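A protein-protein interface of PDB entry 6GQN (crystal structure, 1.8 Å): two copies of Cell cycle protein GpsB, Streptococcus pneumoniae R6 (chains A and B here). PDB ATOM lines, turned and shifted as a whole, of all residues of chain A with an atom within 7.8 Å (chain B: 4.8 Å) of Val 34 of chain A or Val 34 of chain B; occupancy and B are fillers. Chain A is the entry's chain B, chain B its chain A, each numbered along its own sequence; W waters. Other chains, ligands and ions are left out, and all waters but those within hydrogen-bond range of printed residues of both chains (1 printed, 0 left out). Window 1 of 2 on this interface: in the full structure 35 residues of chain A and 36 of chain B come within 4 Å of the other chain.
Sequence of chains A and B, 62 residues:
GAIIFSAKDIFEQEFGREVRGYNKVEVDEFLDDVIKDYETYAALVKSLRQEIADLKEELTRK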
ATOM      1  N   ILE A   4      17.191  -4.466 -24.531  1.00  0.00           N
ATOM      2  CA  ILE A   4      18.642  -4.566 -24.608  1.00  0.00           C
ATOM      3  C   ILE A   4      19.071  -5.474 -25.762  1.00  0.00           C
ATOM      4  O   ILE A   4      19.949  -5.120 -26.563  1.00  0.00           O
ATOM      5  CB  ILE A   4      19.168  -5.063 -23.244  1.00  0.00           C
ATOM      6  CG1 ILE A   4      18.811  -4.021 -22.136  1.00  0.00           C
ATOM      7  CG2 ILE A   4      20.685  -5.285 -23.286  1.00  0.00           C
ATOM      8  CD1 ILE A   4      19.038  -4.495 -20.717  1.00  0.00           C
ATOM      9  N   PHE A   5      18.472  -6.676 -25.843  1.00  0.00           N
ATOM     10  CA  PHE A   5      18.874  -7.748 -26.717  1.00  0.00           C
ATOM     11  C   PHE A   5      17.812  -8.074 -27.751  1.00  0.00           C
ATOM     12  O   PHE A   5      16.617  -7.883 -27.539  1.00  0.00           O
ATOM     13  CB  PHE A   5      19.139  -9.037 -25.928  1.00  0.00           C
ATOM     14  CG  PHE A   5      20.354  -8.972 -25.016  1.00  0.00           C
ATOM     15  CD1 PHE A   5      21.554  -8.471 -25.466  1.00  0.00           C
ATOM     16  CD2 PHE A   5      20.238  -9.348 -23.695  1.00  0.00           C
ATOM     17  CE1 PHE A   5      22.617  -8.365 -24.609  1.00  0.00           C
ATOM     18  CE2 PHE A   5      21.280  -9.282 -22.866  1.00  0.00           C
ATOM     19  CZ  PHE A   5      22.474  -8.803 -23.318  1.00  0.00           C
ATOM     20  N   SER A   6      18.262  -8.655 -28.865  1.00  0.00           N
ATOM     21  CA  SER A   6      17.362  -9.375 -29.756  1.00  0.00           C
ATOM     22  C   SER A   6      17.580 -10.861 -29.549  1.00  0.00           C
ATOM     23  O   SER A   6      18.542 -11.286 -28.905  1.00  0.00           O
ATOM     24  CB  SER A   6      17.680  -9.011 -31.194  1.00  0.00           C
ATOM     25  OG  SER A   6      19.004  -9.476 -31.380  1.00  0.00           O
ATOM     26  N   ALA A   7      16.689 -11.664 -30.123  1.00  0.00           N
ATOM     27  CA  ALA A   7      16.895 -13.106 -30.068  1.00  0.00           C
ATOM     28  C   ALA A   7      18.228 -13.464 -30.684  1.00  0.00           C
ATOM     29  O   ALA A   7      18.955 -14.329 -30.169  1.00  0.00           O
ATOM     30  CB  ALA A   7      15.783 -13.787 -30.827  1.00  0.00           C
ATOM     31  N   ILE A  10      20.960 -13.160 -28.231  1.00  0.00           N
ATOM     32  CA  ILE A  10      21.054 -14.257 -27.276  1.00  0.00           C
ATOM     33  C   ILE A  10      21.756 -15.449 -27.902  1.00  0.00           C
ATOM     34  O   ILE A  10      22.554 -16.124 -27.251  1.00  0.00           O
ATOM     35  CB  ILE A  10      19.660 -14.661 -26.768  1.00  0.00           C
ATOM     36  CG1 ILE A  10      18.868 -13.440 -26.294  1.00  0.00           C
ATOM     37  CG2 ILE A  10      19.765 -15.702 -25.646  1.00  0.00           C
ATOM     38  CD1 ILE A  10      19.567 -12.657 -25.262  1.00  0.00           C
ATOM     39  N   PHE A  11      21.425 -15.761 -29.157  1.00  0.00           N
ATOM     40  CA  PHE A  11      22.086 -16.859 -29.847  1.00  0.00           C
ATOM     41  C   PHE A  11      23.571 -16.571 -30.068  1.00  0.00           C
ATOM     42  O   PHE A  11      24.409 -17.468 -29.961  1.00  0.00           O
ATOM     43  CB  PHE A  11      21.410 -17.074 -31.181  1.00  0.00           C
ATOM     44  CG  PHE A  11      22.096 -18.092 -32.043  1.00  0.00           C
ATOM     45  CD1 PHE A  11      21.799 -19.435 -31.901  1.00  0.00           C
ATOM     46  CD2 PHE A  11      22.949 -17.711 -33.031  1.00  0.00           C
ATOM     47  CE1 PHE A  11      22.433 -20.380 -32.705  1.00  0.00           C
ATOM     48  CE2 PHE A  11      23.547 -18.652 -33.821  1.00  0.00           C
ATOM     49  CZ  PHE A  11      23.267 -19.977 -33.656  1.00  0.00           C
ATOM     50  N   VAL A  27      23.265 -24.146 -19.807  1.00  0.00           N
ATOM     51  CA  VAL A  27      23.031 -22.737 -20.147  1.00  0.00           C
ATOM     52  C   VAL A  27      22.454 -22.603 -21.542  1.00  0.00           C
ATOM     53  O   VAL A  27      21.528 -21.803 -21.793  1.00  0.00           O
ATOM     54  CB  VAL A  27      24.343 -21.939 -20.016  1.00  0.00           C
ATOM     55  CG1 VAL A  27      24.106 -20.550 -20.520  1.00  0.00           C
ATOM     56  CG2 VAL A  27      24.733 -21.877 -18.571  1.00  0.00           C
ATOM     57  N   ASP A  28      23.011 -23.335 -22.489  1.00  0.00           N
ATOM     58  CA  ASP A  28      22.552 -23.209 -23.863  1.00  0.00           C
ATOM     59  C   ASP A  28      21.116 -23.693 -24.012  1.00  0.00           C
ATOM     60  O   ASP A  28      20.326 -23.093 -24.751  1.00  0.00           O
ATOM     61  CB  ASP A  28      23.489 -23.988 -24.789  1.00  0.00           C
ATOM     62  CG  ASP A  28      24.859 -23.307 -25.012  1.00  0.00           C
ATOM     63  OD1 ASP A  28      25.095 -22.159 -24.599  1.00  0.00           O
ATOM     64  OD2 ASP A  28      25.719 -23.949 -25.649  1.00  0.00           O
ATOM     65  N   GLU A  29      20.762 -24.798 -23.362  1.00  0.00           N
ATOM     66  CA  GLU A  29      19.391 -25.291 -23.506  1.00  0.00           C
ATOM     67  C   GLU A  29      18.420 -24.386 -22.804  1.00  0.00           C
ATOM     68  O   GLU A  29      17.272 -24.242 -23.237  1.00  0.00           O
ATOM     69  CB  GLU A  29      19.267 -26.698 -22.959  1.00  0.00           C
ATOM     70  CG  GLU A  29      19.920 -27.660 -23.915  1.00  0.00           C
ATOM     71  CD  GLU A  29      19.843 -29.082 -23.450  1.00  0.00           C
ATOM     72  OE1 GLU A  29      19.260 -29.300 -22.365  1.00  0.00           O
ATOM     73  OE2 GLU A  29      20.376 -29.955 -24.181  1.00  0.00           O
ATOM     74  N   PHE A  30      18.878 -23.721 -21.768  1.00  0.00           N
ATOM     75  CA  PHE A  30      18.061 -22.683 -21.159  1.00  0.00           C
ATOM     76  C   PHE A  30      17.928 -21.473 -22.077  1.00  0.00           C
ATOM     77  O   PHE A  30      16.840 -20.908 -22.222  1.00  0.00           O
ATOM     78  CB  PHE A  30      18.723 -22.309 -19.857  1.00  0.00           C
ATOM     79  CG  PHE A  30      18.131 -21.114 -19.200  1.00  0.00           C
ATOM     80  CD1 PHE A  30      16.959 -21.221 -18.474  1.00  0.00           C
ATOM     81  CD2 PHE A  30      18.768 -19.881 -19.289  1.00  0.00           C
ATOM     82  CE1 PHE A  30      16.408 -20.107 -17.823  1.00  0.00           C
ATOM     83  CE2 PHE A  30      18.219 -18.769 -18.621  1.00  0.00           C
ATOM     84  CZ  PHE A  30      17.026 -18.896 -17.927  1.00  0.00           C
ATOM     85  N   LEU A  31      19.035 -21.043 -22.713  1.00  0.00           N
ATOM     86  CA  LEU A  31      18.968 -19.904 -23.626  1.00  0.00           C
ATOM     87  C   LEU A  31      18.177 -20.216 -24.898  1.00  0.00           C
ATOM     88  O   LEU A  31      17.657 -19.285 -25.542  1.00  0.00           O
ATOM     89  CB  LEU A  31      20.404 -19.462 -23.965  1.00  0.00           C
ATOM     90  CG  LEU A  31      21.147 -18.778 -22.816  1.00  0.00           C
ATOM     91  CD1 LEU A  31      22.574 -18.326 -23.261  1.00  0.00           C
ATOM     92  CD2 LEU A  31      20.369 -17.615 -22.220  1.00  0.00           C
ATOM     93  N   ASP A  32      18.044 -21.495 -25.269  1.00  0.00           N
ATOM     94  CA  ASP A  32      17.121 -21.867 -26.334  1.00  0.00           C
ATOM     95  C   ASP A  32      15.743 -21.303 -26.042  1.00  0.00           C
ATOM     96  O   ASP A  32      15.042 -20.824 -26.931  1.00  0.00           O
ATOM     97  CB  ASP A  32      16.962 -23.381 -26.437  1.00  0.00           C
ATOM     98  CG  ASP A  32      18.172 -24.069 -27.014  1.00  0.00           C
ATOM     99  OD1 ASP A  32      19.108 -23.351 -27.439  1.00  0.00           O
ATOM    100  OD2 ASP A  32      18.128 -25.324 -27.062  1.00  0.00           O
ATOM    101  N   ASP A  33      15.308 -21.461 -24.808  1.00  0.00           N
ATOM    102  CA  ASP A  33      13.956 -21.054 -24.474  1.00  0.00           C
ATOM    103  C   ASP A  33      13.885 -19.545 -24.313  1.00  0.00           C
ATOM    104  O   ASP A  33      12.873 -18.915 -24.670  1.00  0.00           O
ATOM    105  CB  ASP A  33      13.503 -21.785 -23.218  1.00  0.00           C
ATOM    106  CG  ASP A  33      13.099 -23.219 -23.494  1.00  0.00           C
ATOM    107  OD1 ASP A  33      12.927 -23.626 -24.680  1.00  0.00           O
ATOM    108  OD2 ASP A  33      12.917 -23.937 -22.493  1.00  0.00           O
ATOM    109  N   VAL A  34      14.955 -18.939 -23.783  1.00  0.00           N
ATOM    110  CA  VAL A  34      15.025 -17.478 -23.720  1.00  0.00           C
ATOM    111  C   VAL A  34      14.898 -16.903 -25.116  1.00  0.00           C
ATOM    112  O   VAL A  34      14.152 -15.942 -25.357  1.00  0.00           O
ATOM    113  CB  VAL A  34      16.348 -17.038 -23.039  1.00  0.00           C
ATOM    114  CG1 VAL A  34      16.570 -15.488 -23.190  1.00  0.00           C
ATOM    115  CG2 VAL A  34      16.269 -17.359 -21.566  1.00  0.00           C
ATOM    116  N   ILE A  35      15.647 -17.471 -26.068  1.00  0.00           N
ATOM    117  CA  ILE A  35      15.549 -17.034 -27.444  1.00  0.00           C
ATOM    118  C   ILE A  35      14.116 -17.146 -27.947  1.00  0.00           C
ATOM    119  O   ILE A  35      13.615 -16.263 -28.653  1.00  0.00           O
ATOM    120  CB  ILE A  35      16.499 -17.870 -28.297  1.00  0.00           C
ATOM    121  CG1 ILE A  35      17.922 -17.402 -28.029  1.00  0.00           C
ATOM    122  CG2 ILE A  35      16.139 -17.804 -29.763  1.00  0.00           C
ATOM    123  CD1 ILE A  35      18.997 -18.503 -28.566  1.00  0.00           C
ATOM    124  N   LYS A  36      13.465 -18.262 -27.672  1.00  0.00           N
ATOM    125  CA  LYS A  36      12.088 -18.392 -28.169  1.00  0.00           C
ATOM    126  C   LYS A  36      11.190 -17.320 -27.579  1.00  0.00           C
ATOM    127  O   LYS A  36      10.277 -16.822 -28.263  1.00  0.00           O
ATOM    128  CB  LYS A  36      11.523 -19.758 -27.825  1.00  0.00           C
ATOM    129  CG  LYS A  36      12.155 -20.902 -28.574  1.00  0.00           C
ATOM    130  CD  LYS A  36      11.579 -22.172 -28.026  1.00  0.00           C
ATOM    131  CE  LYS A  36      12.018 -23.378 -28.820  1.00  0.00           C
ATOM    132  NZ  LYS A  36      11.692 -24.622 -28.088  1.00  0.00           N
ATOM    133  N   ASP A  37      11.452 -16.909 -26.339  1.00  0.00           N
ATOM    134  CA  ASP A  37      10.634 -15.847 -25.751  1.00  0.00           C
ATOM    135  C   ASP A  37      10.985 -14.510 -26.359  1.00  0.00           C
ATOM    136  O   ASP A  37      10.108 -13.660 -26.531  1.00  0.00           O
ATOM    137  CB  ASP A  37      10.819 -15.763 -24.248  1.00  0.00           C
ATOM    138  CG  ASP A  37      10.107 -16.828 -23.508  1.00  0.00           C
ATOM    139  OD1 ASP A  37       9.153 -17.476 -24.066  1.00  0.00           O
ATOM    140  OD2 ASP A  37      10.433 -16.989 -22.308  1.00  0.00           O
ATOM    141  N   TYR A  38      12.269 -14.272 -26.660  1.00  0.00           N
ATOM    142  CA  TYR A  38      12.592 -13.031 -27.348  1.00  0.00           C
ATOM    143  C   TYR A  38      11.899 -12.954 -28.684  1.00  0.00           C
ATOM    144  O   TYR A  38      11.374 -11.905 -29.048  1.00  0.00           O
ATOM    145  CB  TYR A  38      14.069 -12.908 -27.563  1.00  0.00           C
ATOM    146  CG  TYR A  38      14.742 -12.180 -26.462  1.00  0.00           C
ATOM    147  CD1 TYR A  38      15.218 -12.879 -25.365  1.00  0.00           C
ATOM    148  CD2 TYR A  38      14.924 -10.786 -26.523  1.00  0.00           C
ATOM    149  CE1 TYR A  38      15.889 -12.233 -24.346  1.00  0.00           C
ATOM    150  CE2 TYR A  38      15.536 -10.150 -25.529  1.00  0.00           C
ATOM    151  CZ  TYR A  38      16.047 -10.861 -24.450  1.00  0.00           C
ATOM    152  OH  TYR A  38      16.714 -10.207 -23.480  1.00  0.00           O
ATOM    153  N   GLU A  39      11.862 -14.069 -29.427  1.00  0.00           N
ATOM    154  CA  GLU A  39      11.140 -14.055 -30.685  1.00  0.00           C
ATOM    155  C   GLU A  39       9.659 -13.803 -30.466  1.00  0.00           C
ATOM    156  O   GLU A  39       9.039 -13.013 -31.200  1.00  0.00           O
ATOM    157  CB  GLU A  39      11.326 -15.380 -31.408  1.00  0.00           C
ATOM    158  CG  GLU A  39      12.785 -15.584 -31.737  1.00  0.00           C
ATOM    159  CD  GLU A  39      12.992 -16.615 -32.795  1.00  0.00           C
ATOM    160  OE1 GLU A  39      13.048 -17.800 -32.442  1.00  0.00           O
ATOM    161  OE2 GLU A  39      13.079 -16.238 -33.974  1.00  0.00           O
ATOM    162  N   THR A  40       9.065 -14.499 -29.495  1.00  0.00           N
ATOM    163  CA  THR A  40       7.632 -14.347 -29.237  1.00  0.00           C
ATOM    164  C   THR A  40       7.313 -12.930 -28.806  1.00  0.00           C
ATOM    165  O   THR A  40       6.391 -12.286 -29.353  1.00  0.00           O
ATOM    166  CB  THR A  40       7.212 -15.333 -28.166  1.00  0.00           C
ATOM    167  OG1 THR A  40       7.402 -16.659 -28.661  1.00  0.00           O
ATOM    168  CG2 THR A  40       5.750 -15.194 -27.853  1.00  0.00           C
ATOM    169  N   TYR A  41       8.091 -12.400 -27.843  1.00  0.00           N
ATOM    170  CA  TYR A  41       7.845 -11.038 -27.377  1.00  0.00           C
ATOM    171  C   TYR A  41       8.024 -10.002 -28.481  1.00  0.00           C
ATOM    172  O   TYR A  41       7.222  -9.058 -28.586  1.00  0.00           O
ATOM    173  CB  TYR A  41       8.758 -10.706 -26.188  1.00  0.00           C
ATOM    174  CG  TYR A  41       8.174 -10.984 -24.813  1.00  0.00           C
ATOM    175  CD1 TYR A  41       6.873 -10.556 -24.470  1.00  0.00           C
ATOM    176  CD2 TYR A  41       8.906 -11.644 -23.843  1.00  0.00           C
ATOM    177  CE1 TYR A  41       6.353 -10.804 -23.190  1.00  0.00           C
ATOM    178  CE2 TYR A  41       8.362 -11.900 -22.561  1.00  0.00           C
ATOM    179  CZ  TYR A  41       7.093 -11.472 -22.259  1.00  0.00           C
ATOM    180  OH  TYR A  41       6.557 -11.700 -21.044  1.00  0.00           O
ATOM    181  N   PHE B   5       9.095 -18.264 -20.039  1.00  0.00           N
ATOM    182  CA  PHE B   5       9.632 -17.825 -18.770  1.00  0.00           C
ATOM    183  C   PHE B   5       9.042 -16.486 -18.361  1.00  0.00           C
ATOM    184  O   PHE B   5       8.632 -15.689 -19.188  1.00  0.00           O
ATOM    185  CB  PHE B   5      11.129 -17.624 -18.869  1.00  0.00           C
ATOM    186  CG  PHE B   5      11.900 -18.877 -19.041  1.00  0.00           C
ATOM    187  CD1 PHE B   5      11.638 -19.973 -18.245  1.00  0.00           C
ATOM    188  CD2 PHE B   5      12.949 -18.945 -19.999  1.00  0.00           C
ATOM    189  CE1 PHE B   5      12.368 -21.133 -18.421  1.00  0.00           C
ATOM    190  CE2 PHE B   5      13.676 -20.138 -20.156  1.00  0.00           C
ATOM    191  CZ  PHE B   5      13.384 -21.206 -19.353  1.00  0.00           C
ATOM    192  N   ILE B  10      14.144 -16.269 -14.871  1.00  0.00           N
ATOM    193  CA  ILE B  10      15.510 -15.956 -15.268  1.00  0.00           C
ATOM    194  C   ILE B  10      16.334 -15.745 -14.031  1.00  0.00           C
ATOM    195  O   ILE B  10      17.468 -16.221 -13.931  1.00  0.00           O
ATOM    196  CB  ILE B  10      15.543 -14.726 -16.208  1.00  0.00           C
ATOM    197  CG1 ILE B  10      14.501 -14.884 -17.352  1.00  0.00           C
ATOM    198  CG2 ILE B  10      16.970 -14.515 -16.847  1.00  0.00           C
ATOM    199  CD1 ILE B  10      14.704 -16.148 -18.141  1.00  0.00           C
ATOM    200  N   PHE B  30      25.017 -11.198 -18.017  1.00  0.00           N
ATOM    201  CA  PHE B  30      24.210 -11.283 -19.217  1.00  0.00           C
ATOM    202  C   PHE B  30      22.763 -11.526 -18.850  1.00  0.00           C
ATOM    203  O   PHE B  30      21.859 -10.821 -19.329  1.00  0.00           O
ATOM    204  CB  PHE B  30      24.760 -12.419 -20.086  1.00  0.00           C
ATOM    205  CG  PHE B  30      23.927 -12.728 -21.278  1.00  0.00           C
ATOM    206  CD1 PHE B  30      23.900 -11.879 -22.375  1.00  0.00           C
ATOM    207  CD2 PHE B  30      23.187 -13.890 -21.326  1.00  0.00           C
ATOM    208  CE1 PHE B  30      23.147 -12.206 -23.478  1.00  0.00           C
ATOM    209  CE2 PHE B  30      22.474 -14.216 -22.421  1.00  0.00           C
ATOM    210  CZ  PHE B  30      22.425 -13.358 -23.482  1.00  0.00           C
ATOM    211  N   LEU B  31      22.518 -12.540 -17.993  1.00  0.00           N
ATOM    212  CA  LEU B  31      21.139 -12.851 -17.600  1.00  0.00           C
ATOM    213  C   LEU B  31      20.490 -11.684 -16.862  1.00  0.00           C
ATOM    214  O   LEU B  31      19.263 -11.583 -16.821  1.00  0.00           O
ATOM    215  CB  LEU B  31      21.111 -14.100 -16.704  1.00  0.00           C
ATOM    216  CG  LEU B  31      21.448 -15.330 -17.547  1.00  0.00           C
ATOM    217  CD1 LEU B  31      21.417 -16.617 -16.709  1.00  0.00           C
ATOM    218  CD2 LEU B  31      20.498 -15.457 -18.735  1.00  0.00           C
ATOM    219  N   ASP B  32      21.272 -10.847 -16.205  1.00  0.00           N
ATOM    220  CA  ASP B  32      20.661  -9.722 -15.523  1.00  0.00           C
ATOM    221  C   ASP B  32      20.063  -8.779 -16.525  1.00  0.00           C
ATOM    222  O   ASP B  32      19.064  -8.144 -16.239  1.00  0.00           O
ATOM    223  CB  ASP B  32      21.678  -8.954 -14.689  1.00  0.00           C
ATOM    224  CG  ASP B  32      21.921  -9.569 -13.323  1.00  0.00           C
ATOM    225  OD1 ASP B  32      21.077 -10.373 -12.851  1.00  0.00           O
ATOM    226  OD2 ASP B  32      22.980  -9.239 -12.723  1.00  0.00           O
ATOM    227  N   ASP B  33      20.669  -8.695 -17.713  1.00  0.00           N
ATOM    228  CA  ASP B  33      20.110  -7.869 -18.764  1.00  0.00           C
ATOM    229  C   ASP B  33      18.905  -8.540 -19.370  1.00  0.00           C
ATOM    230  O   ASP B  33      17.942  -7.884 -19.760  1.00  0.00           O
ATOM    231  CB  ASP B  33      21.166  -7.615 -19.824  1.00  0.00           C
ATOM    232  CG  ASP B  33      22.087  -6.475 -19.442  1.00  0.00           C
ATOM    233  OD1 ASP B  33      21.880  -5.857 -18.379  1.00  0.00           O
ATOM    234  OD2 ASP B  33      23.022  -6.214 -20.207  1.00  0.00           O
ATOM    235  N   VAL B  34      18.956  -9.868 -19.456  1.00  0.00           N
ATOM    236  CA  VAL B  34      17.798 -10.613 -19.925  1.00  0.00           C
ATOM    237  C   VAL B  34      16.633 -10.393 -18.971  1.00  0.00           C
ATOM    238  O   VAL B  34      15.504 -10.130 -19.389  1.00  0.00           O
ATOM    239  CB  VAL B  34      18.163 -12.096 -20.067  1.00  0.00           C
ATOM    240  CG1 VAL B  34      16.860 -12.926 -20.362  1.00  0.00           C
ATOM    241  CG2 VAL B  34      19.154 -12.244 -21.209  1.00  0.00           C
ATOM    242  N   ILE B  35      16.899 -10.436 -17.683  1.00  0.00           N
ATOM    243  CA  ILE B  35      15.838 -10.142 -16.726  1.00  0.00           C
ATOM    244  C   ILE B  35      15.210  -8.802 -17.049  1.00  0.00           C
ATOM    245  O   ILE B  35      13.979  -8.637 -17.020  1.00  0.00           O
ATOM    246  CB  ILE B  35      16.429 -10.143 -15.318  1.00  0.00           C
ATOM    247  CG1 ILE B  35      16.813 -11.597 -14.977  1.00  0.00           C
ATOM    248  CG2 ILE B  35      15.458  -9.526 -14.303  1.00  0.00           C
ATOM    249  CD1 ILE B  35      17.488 -11.685 -13.670  1.00  0.00           C
ATOM    250  N   LYS B  36      16.039  -7.815 -17.308  1.00  0.00           N
ATOM    251  CA  LYS B  36      15.475  -6.486 -17.551  1.00  0.00           C
ATOM    252  C   LYS B  36      14.597  -6.500 -18.788  1.00  0.00           C
ATOM    253  O   LYS B  36      13.527  -5.853 -18.829  1.00  0.00           O
ATOM    254  CB  LYS B  36      16.592  -5.441 -17.677  1.00  0.00           C
ATOM    255  CG  LYS B  36      17.344  -5.106 -16.408  1.00  0.00           C
ATOM    256  CD  LYS B  36      18.501  -4.116 -16.773  1.00  0.00           C
ATOM    257  CE  LYS B  36      19.604  -4.083 -15.742  1.00  0.00           C
ATOM    258  NZ  LYS B  36      20.548  -2.995 -16.059  1.00  0.00           N
ATOM    259  N   ASP B  37      15.028  -7.218 -19.826  1.00  0.00           N
ATOM    260  CA  ASP B  37      14.233  -7.347 -21.043  1.00  0.00           C
ATOM    261  C   ASP B  37      12.924  -8.063 -20.807  1.00  0.00           C
ATOM    262  O   ASP B  37      11.904  -7.706 -21.408  1.00  0.00           O
ATOM    263  CB  ASP B  37      15.013  -8.075 -22.146  1.00  0.00           C
ATOM    264  CG  ASP B  37      16.016  -7.140 -22.866  1.00  0.00           C
ATOM    265  OD1 ASP B  37      15.966  -5.878 -22.625  1.00  0.00           O
ATOM    266  OD2 ASP B  37      16.877  -7.638 -23.632  1.00  0.00           O
ATOM    267  N   TYR B  38      12.922  -9.112 -19.994  1.00  0.00           N
ATOM    268  CA  TYR B  38      11.649  -9.751 -19.706  1.00  0.00           C
ATOM    269  C   TYR B  38      10.746  -8.809 -18.925  1.00  0.00           C
ATOM    270  O   TYR B  38       9.540  -8.758 -19.162  1.00  0.00           O
ATOM    271  CB  TYR B  38      11.869 -11.008 -18.892  1.00  0.00           C
ATOM    272  CG  TYR B  38      12.059 -12.262 -19.680  1.00  0.00           C
ATOM    273  CD1 TYR B  38      13.289 -12.567 -20.240  1.00  0.00           C
ATOM    274  CD2 TYR B  38      11.004 -13.168 -19.833  1.00  0.00           C
ATOM    275  CE1 TYR B  38      13.490 -13.764 -20.905  1.00  0.00           C
ATOM    276  CE2 TYR B  38      11.170 -14.318 -20.518  1.00  0.00           C
ATOM    277  CZ  TYR B  38      12.450 -14.622 -21.030  1.00  0.00           C
ATOM    278  OH  TYR B  38      12.596 -15.781 -21.711  1.00  0.00           O
HETATM  279  O   HOH W   1       7.302 -13.174 -19.045  1.00  0.00           O
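The side-chain hydroxyl of Tyr 38 of chain B lies within hydrogen-bond range of the side-chain carboxylate of Asp 37 of chain A, at 2.5 Å. OD2 of Asp 37 of chain B lies within hydrogen-bond range of N of Phe 5 of chain A (2.9 Å). The backbone NH (N) of Ile 4 of chain A is in hydrogen-bond range of the side-chain carboxylate (OD1) of Asp 37 of chain B, at 2.7 Å. The backbone NH (N) of Phe 5 of chain B sits at hydrogen-bond distance from the side-chain carboxylate (OD2) of Asp 37 of chain A, 2.9 Å away. The side-chain carboxylate (OD2) of Asp 37 of chain B is in hydrogen-bond range of the side-chain hydroxyl (OH) of Tyr 38 of chain A.
The side-chain carboxylate (OD1) of Asp 33 of chain B lies within salt-bridge range of the side-chain amino group (NZ) of Lys 36 of chain B (3.9 Å). OD1 of Asp 33 of chain A is in salt-bridge range of NZ of Lys 36 of chain A (3.8 Å).
Among the printed residues, pairs that only touch across the chains: Ile 4 of chain A with Asp 33 of chain B, Ile 4 of chain A with Lys 36 of chain B, Phe 5 of chain A with Phe 30 of chain B, Phe 5 of chain A with Asp 33 of chain B, Phe 5 of chain A with Val 34 of chain B, Ile 10 of chain A with Phe 30 of chain B, Phe 30 of chain A with Phe 5 of chain B, Phe 30 of chain A with Ile 10 of chain B, Asp 33 of chain A with Phe 5 of chain B, Val 34 of chain A with Phe 5 of chain B, Val 34 of chain A with Ile 10 of chain B, Val 34 of chain A with Val 34 of chain B, Val 34 of chain A with Tyr 38 of chain B and Tyr 38 of chain A with Val 34 of chain B.
Of the printed residues of chain B, Val 34 of chain A touches Phe 5, Ile 10, Val 34 and Tyr 38. Of chain A, only Phe 5 (3.97 Å), Val 34 (3.8 Å) and Tyr 38 (3.7 Å) come within 4 Å of Val 34 of chain B. Printed residues of chain A within 4 Å of Phe 5 of chain B: Phe 30, Asp 33, Val 34 and Asp 37. Printed residues of chain B within 4 Å of Asp 33 of chain A: Phe 5. Of the printed residues of chain B, Phe 5 of chain A touches Phe 30, Asp 33, Val 34 and Asp 37. Of the printed residues of chain A, Tyr 38 of chain B touches Val 34 (3.6 Å) and Asp 37 (2.5 Å). Of the printed residues of chain B, Ile 4 of chain A touches Asp 33 (3.7 Å), Lys 36 (3.998 Å) and Asp 37 (2.7 Å). Glu 39 of chain A touches none of the printed residues of chain B. The nearest printed residue of chain A that does not touch Asp 33 of chain B is Tyr 38 of chain A (4.6 Å).
Hydrophobic or aromatic side chains of chain A within 4 Å of the printed part of chain B: Ile 4, Phe 5, Ile 10, Phe 30, Val 34 and Tyr 38. Among the printed residues, no Asp or Glu carboxylate lies within 4 Å of a Lys or Arg side-chain nitrogen of the other chain.
Phe 5 of chain A touches Phe 30 of chain B, and with the chains exchanged Phe 30 of chain A touches Phe 5 of chain B. Phe 5 of chain A touches Asp 33 of chain B, and with the chains exchanged Asp 33 of chain A touches Phe 5 of chain B. Phe 5 of chain A touches Val 34 of chain B, and with the chains exchanged Val 34 of chain A touches Phe 5 of chain B. Val 34 of chain A touches Ile 10 of chain B, but with the chains exchanged Ile 10 of chain A does not touch Val 34 of chain B (4.1 Å). Positions printed for both chains: 5, 10, 30, 31, 32, 33, 34, 35, 36, 37 and 38.
Water W1 lies within hydrogen-bond range of OH of Tyr 41 of chain A and O of Phe 5 of chain B.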
